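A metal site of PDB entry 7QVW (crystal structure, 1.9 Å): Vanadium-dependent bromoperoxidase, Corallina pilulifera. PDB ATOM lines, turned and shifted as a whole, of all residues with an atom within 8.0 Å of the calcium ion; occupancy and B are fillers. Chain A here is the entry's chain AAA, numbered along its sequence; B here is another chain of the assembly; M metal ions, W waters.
O of Gln 370 binds the calcium ion (2.3 Å).
OD2 of Asp 368 binds the calcium ion (2.4 Å).
The calcium ion is bound by O of Gln 363 (2.4 Å).
O of Phe 361 binds the calcium ion, 2.5 Å away.
The calcium ion is bound by the side-chain carboxylate (OD1) of Asp 365, at 2.5 Å.
Water W1 binds the calcium ion (2.5 Å).
The calcium ion is bound by OD1 of Asp 368 (2.6 Å).
The calcium ion has seven donor atoms within binding distance.
O of Trp 125 of chain B lies close to NE2 of Gln 370, at 3.3 Å.
The backbone carbonyl oxygen of Asp 365 lies close to the side-chain amide oxygen of Asn 369, 3.5 Å away.
The backbone NH (N) of Gly 124 of chain B sits at hydrogen-bond distance from the side-chain carboxylate (OD2) of Asp 365 (2.7 Å).
Within 4 Å of the calcium ion: Phe 361, Gln 363, Asp 365, Asp 368 and Gln 370.
The nearest printed residue that does not touch the calcium ion is Gln 362 (4.2 Å).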
ATOM      1  N   PRO A 360      32.815  -6.992  11.371  1.00  0.00           N
ATOM      2  CA  PRO A 360      32.004  -7.873  12.203  1.00  0.00           C
ATOM      3  C   PRO A 360      31.290  -7.081  13.295  1.00  0.00           C
ATOM      4  O   PRO A 360      31.735  -5.979  13.638  1.00  0.00           O
ATOM      5  CB  PRO A 360      33.041  -8.780  12.945  1.00  0.00           C
ATOM      6  CG  PRO A 360      34.351  -8.559  12.197  1.00  0.00           C
ATOM      7  CD  PRO A 360      34.260  -7.132  11.682  1.00  0.00           C
ATOM      8  N   PHE A 361      30.216  -7.680  13.824  1.00  0.00           N
ATOM      9  CA  PHE A 361      29.620  -7.290  15.103  1.00  0.00           C
ATOM     10  C   PHE A 361      28.875  -5.943  14.983  1.00  0.00           C
ATOM     11  O   PHE A 361      28.583  -5.311  15.979  1.00  0.00           O
ATOM     12  CB  PHE A 361      30.681  -7.243  16.209  1.00  0.00           C
ATOM     13  CG  PHE A 361      31.449  -8.526  16.353  1.00  0.00           C
ATOM     14  CD1 PHE A 361      30.795  -9.760  16.311  1.00  0.00           C
ATOM     15  CD2 PHE A 361      32.821  -8.521  16.613  1.00  0.00           C
ATOM     16  CE1 PHE A 361      31.483 -10.962  16.486  1.00  0.00           C
ATOM     17  CE2 PHE A 361      33.516  -9.711  16.753  1.00  0.00           C
ATOM     18  CZ  PHE A 361      32.861 -10.935  16.697  1.00  0.00           C
ATOM     19  N   GLN A 362      28.588  -5.488  13.776  1.00  0.00           N
ATOM     20  CA  GLN A 362      27.974  -4.182  13.630  1.00  0.00           C
ATOM     21  C   GLN A 362      26.433  -4.243  13.748  1.00  0.00           C
ATOM     22  O   GLN A 362      25.775  -3.219  13.609  1.00  0.00           O
ATOM     23  CB  GLN A 362      28.408  -3.543  12.317  1.00  0.00           C
ATOM     24  CG  GLN A 362      29.928  -3.435  12.172  1.00  0.00           C
ATOM     25  CD  GLN A 362      30.621  -2.625  13.240  1.00  0.00           C
ATOM     26  OE1 GLN A 362      30.071  -1.639  13.754  1.00  0.00           O
ATOM     27  NE2 GLN A 362      31.840  -3.039  13.557  1.00  0.00           N
ATOM     28  N   GLN A 363      25.849  -5.427  13.992  1.00  0.00           N
ATOM     29  CA  GLN A 363      24.410  -5.538  14.114  1.00  0.00           C
ATOM     30  C   GLN A 363      24.002  -5.156  15.531  1.00  0.00           C
ATOM     31  O   GLN A 363      24.834  -5.048  16.426  1.00  0.00           O
ATOM     32  CB  GLN A 363      23.969  -6.978  13.863  1.00  0.00           C
ATOM     33  CG  GLN A 363      24.213  -7.396  12.408  1.00  0.00           C
ATOM     34  CD  GLN A 363      23.818  -8.831  12.223  1.00  0.00           C
ATOM     35  OE1 GLN A 363      22.654  -9.123  11.947  1.00  0.00           O
ATOM     36  NE2 GLN A 363      24.759  -9.737  12.472  1.00  0.00           N
ATOM     37  N   GLU A 364      22.695  -4.976  15.747  1.00  0.00           N
ATOM     38  CA  GLU A 364      22.210  -4.793  17.100  1.00  0.00           C
ATOM     39  C   GLU A 364      22.649  -5.974  17.956  1.00  0.00           C
ATOM     40  O   GLU A 364      22.640  -7.112  17.501  1.00  0.00           O
ATOM     41  CB  GLU A 364      20.682  -4.725  17.096  1.00  0.00           C
ATOM     42  CG  GLU A 364      20.199  -3.520  16.312  1.00  0.00           C
ATOM     43  CD  GLU A 364      18.723  -3.233  16.499  1.00  0.00           C
ATOM     44  OE1 GLU A 364      18.018  -4.053  17.166  1.00  0.00           O
ATOM     45  OE2 GLU A 364      18.273  -2.173  15.973  1.00  0.00           O
ATOM     46  N   ASP A 365      23.000  -5.692  19.210  1.00  0.00           N
ATOM     47  CA  ASP A 365      23.615  -6.687  20.070  1.00  0.00           C
ATOM     48  C   ASP A 365      22.638  -7.824  20.394  1.00  0.00           C
ATOM     49  O   ASP A 365      23.082  -8.937  20.663  1.00  0.00           O
ATOM     50  CB  ASP A 365      24.213  -6.091  21.339  1.00  0.00           C
ATOM     51  CG  ASP A 365      25.423  -5.217  21.014  1.00  0.00           C
ATOM     52  OD1 ASP A 365      25.829  -5.219  19.871  1.00  0.00           O
ATOM     53  OD2 ASP A 365      25.966  -4.564  21.903  1.00  0.00           O
ATOM     54  N   LYS A 366      21.323  -7.554  20.310  1.00  0.00           N
ATOM     55  CA  LYS A 366      20.406  -8.670  20.529  1.00  0.00           C
ATOM     56  C   LYS A 366      20.575  -9.727  19.439  1.00  0.00           C
ATOM     57  O   LYS A 366      20.260 -10.877  19.659  1.00  0.00           O
ATOM     58  CB  LYS A 366      18.931  -8.248  20.529  1.00  0.00           C
ATOM     59  CG  LYS A 366      18.451  -7.644  19.224  1.00  0.00           C
ATOM     60  CD  LYS A 366      17.001  -7.138  19.284  1.00  0.00           C
ATOM     61  CE  LYS A 366      16.470  -6.754  17.904  1.00  0.00           C
ATOM     62  NZ  LYS A 366      15.588  -5.560  17.890  1.00  0.00           N
ATOM     63  N   LEU A 367      21.138  -9.342  18.279  1.00  0.00           N
ATOM     64  CA  LEU A 367      21.369 -10.308  17.231  1.00  0.00           C
ATOM     65  C   LEU A 367      22.762 -10.951  17.332  1.00  0.00           C
ATOM     66  O   LEU A 367      22.888 -12.173  17.180  1.00  0.00           O
ATOM     67  CB  LEU A 367      21.173  -9.625  15.870  1.00  0.00           C
ATOM     68  CG  LEU A 367      19.766  -9.065  15.635  1.00  0.00           C
ATOM     69  CD1 LEU A 367      19.661  -8.443  14.248  1.00  0.00           C
ATOM     70  CD2 LEU A 367      18.715 -10.167  15.752  1.00  0.00           C
ATOM     71  N   ASP A 368      23.809 -10.146  17.578  1.00  0.00           N
ATOM     72  CA  ASP A 368      25.160 -10.692  17.466  1.00  0.00           C
ATOM     73  C   ASP A 368      25.851 -10.908  18.823  1.00  0.00           C
ATOM     74  O   ASP A 368      26.947 -11.483  18.861  1.00  0.00           O
ATOM     75  CB  ASP A 368      26.043  -9.851  16.517  1.00  0.00           C
ATOM     76  CG  ASP A 368      26.184  -8.391  16.930  1.00  0.00           C
ATOM     77  OD1 ASP A 368      25.881  -8.081  18.096  1.00  0.00           O
ATOM     78  OD2 ASP A 368      26.639  -7.561  16.087  1.00  0.00           O
ATOM     79  N   ASN A 369      25.238 -10.454  19.933  1.00  0.00           N
ATOM     80  CA  ASN A 369      25.805 -10.570  21.268  1.00  0.00           C
ATOM     81  C   ASN A 369      27.201  -9.939  21.340  1.00  0.00           C
ATOM     82  O   ASN A 369      28.024 -10.377  22.148  1.00  0.00           O
ATOM     83  CB  ASN A 369      25.944 -12.025  21.765  1.00  0.00           C
ATOM     84  CG  ASN A 369      24.611 -12.722  21.950  1.00  0.00           C
ATOM     85  OD1 ASN A 369      23.587 -12.069  22.053  1.00  0.00           O
ATOM     86  ND2 ASN A 369      24.588 -14.040  21.948  1.00  0.00           N
ATOM     87  N   GLN A 370      27.466  -8.896  20.527  1.00  0.00           N
ATOM     88  CA  GLN A 370      28.843  -8.421  20.519  1.00  0.00           C
ATOM     89  C   GLN A 370      28.899  -6.954  20.102  1.00  0.00           C
ATOM     90  O   GLN A 370      28.492  -6.588  19.003  1.00  0.00           O
ATOM     91  CB  GLN A 370      29.674  -9.264  19.539  1.00  0.00           C
ATOM     92  CG  GLN A 370      31.177  -9.034  19.713  1.00  0.00           C
ATOM     93  CD  GLN A 370      31.883  -9.801  20.818  1.00  0.00           C
ATOM     94  OE1 GLN A 370      33.104  -9.776  20.888  1.00  0.00           O
ATOM     95  NE2 GLN A 370      31.151 -10.491  21.695  1.00  0.00           N
ATOM     96  N   ASP A 371      29.479  -6.130  20.964  1.00  0.00           N
ATOM     97  CA  ASP A 371      29.719  -4.727  20.659  1.00  0.00           C
ATOM     98  C   ASP A 371      31.210  -4.610  20.341  1.00  0.00           C
ATOM     99  O   ASP A 371      31.967  -5.572  20.461  1.00  0.00           O
ATOM    100  CB  ASP A 371      29.342  -3.890  21.889  1.00  0.00           C
ATOM    101  CG  ASP A 371      29.195  -2.392  21.672  1.00  0.00           C
ATOM    102  OD1 ASP A 371      29.384  -1.934  20.545  1.00  0.00           O
ATOM    103  OD2 ASP A 371      28.876  -1.689  22.664  1.00  0.00           O
ATOM    104  N   VAL A 372      31.625  -3.422  19.889  1.00  0.00           N
ATOM    105  CA  VAL A 372      32.959  -3.270  19.312  1.00  0.00           C
ATOM    106  C   VAL A 372      33.703  -2.145  20.027  1.00  0.00           C
ATOM    107  O   VAL A 372      33.097  -1.133  20.413  1.00  0.00           O
ATOM    108  CB  VAL A 372      32.879  -3.002  17.794  1.00  0.00           C
ATOM    109  CG1 VAL A 372      32.457  -4.283  17.066  1.00  0.00           C
ATOM    110  CG2 VAL A 372      31.947  -1.832  17.446  1.00  0.00           C
ATOM    111  N   ARG B 123      22.829  -4.883  25.679  1.00  0.00           N
ATOM    112  CA  ARG B 123      24.102  -4.561  25.033  1.00  0.00           C
ATOM    113  C   ARG B 123      24.998  -5.785  25.131  1.00  0.00           C
ATOM    114  O   ARG B 123      24.814  -6.584  26.057  1.00  0.00           O
ATOM    115  CB  ARG B 123      24.780  -3.394  25.770  1.00  0.00           C
ATOM    116  CG  ARG B 123      25.011  -3.695  27.251  1.00  0.00           C
ATOM    117  CD  ARG B 123      25.713  -2.514  27.903  1.00  0.00           C
ATOM    118  NE  ARG B 123      26.992  -2.239  27.294  1.00  0.00           N
ATOM    119  CZ  ARG B 123      27.949  -1.456  27.820  1.00  0.00           C
ATOM    120  NH1 ARG B 123      27.754  -0.905  29.008  1.00  0.00           N
ATOM    121  NH2 ARG B 123      29.073  -1.259  27.134  1.00  0.00           N
ATOM    122  N   GLY B 124      25.959  -5.940  24.199  1.00  0.00           N
ATOM    123  CA  GLY B 124      26.732  -7.184  24.132  1.00  0.00           C
ATOM    124  C   GLY B 124      28.194  -7.004  24.569  1.00  0.00           C
ATOM    125  O   GLY B 124      28.663  -5.876  24.770  1.00  0.00           O
ATOM    126  N   TRP B 125      28.919  -8.117  24.699  1.00  0.00           N
ATOM    127  CA  TRP B 125      30.313  -8.051  25.142  1.00  0.00           C
ATOM    128  C   TRP B 125      31.144  -7.294  24.097  1.00  0.00           C
ATOM    129  O   TRP B 125      30.907  -7.375  22.879  1.00  0.00           O
ATOM    130  CB  TRP B 125      30.813  -9.475  25.395  1.00  0.00           C
ATOM    131  CG  TRP B 125      29.988 -10.111  26.487  1.00  0.00           C
ATOM    132  CD1 TRP B 125      30.085  -9.838  27.812  1.00  0.00           C
ATOM    133  CD2 TRP B 125      28.944 -11.098  26.350  1.00  0.00           C
ATOM    134  NE1 TRP B 125      29.198 -10.624  28.533  1.00  0.00           N
ATOM    135  CE2 TRP B 125      28.462 -11.373  27.653  1.00  0.00           C
ATOM    136  CE3 TRP B 125      28.371 -11.764  25.251  1.00  0.00           C
ATOM    137  CZ2 TRP B 125      27.426 -12.267  27.897  1.00  0.00           C
ATOM    138  CZ3 TRP B 125      27.333 -12.645  25.492  1.00  0.00           C
ATOM    139  CH2 TRP B 125      26.893 -12.915  26.787  1.00  0.00           C
HETATM  140 CA    CA M   1      26.812  -5.721  17.628  1.00  0.00          CA
HETATM  141  O   HOH W   1      27.459  -3.277  17.775  1.00  0.00           O
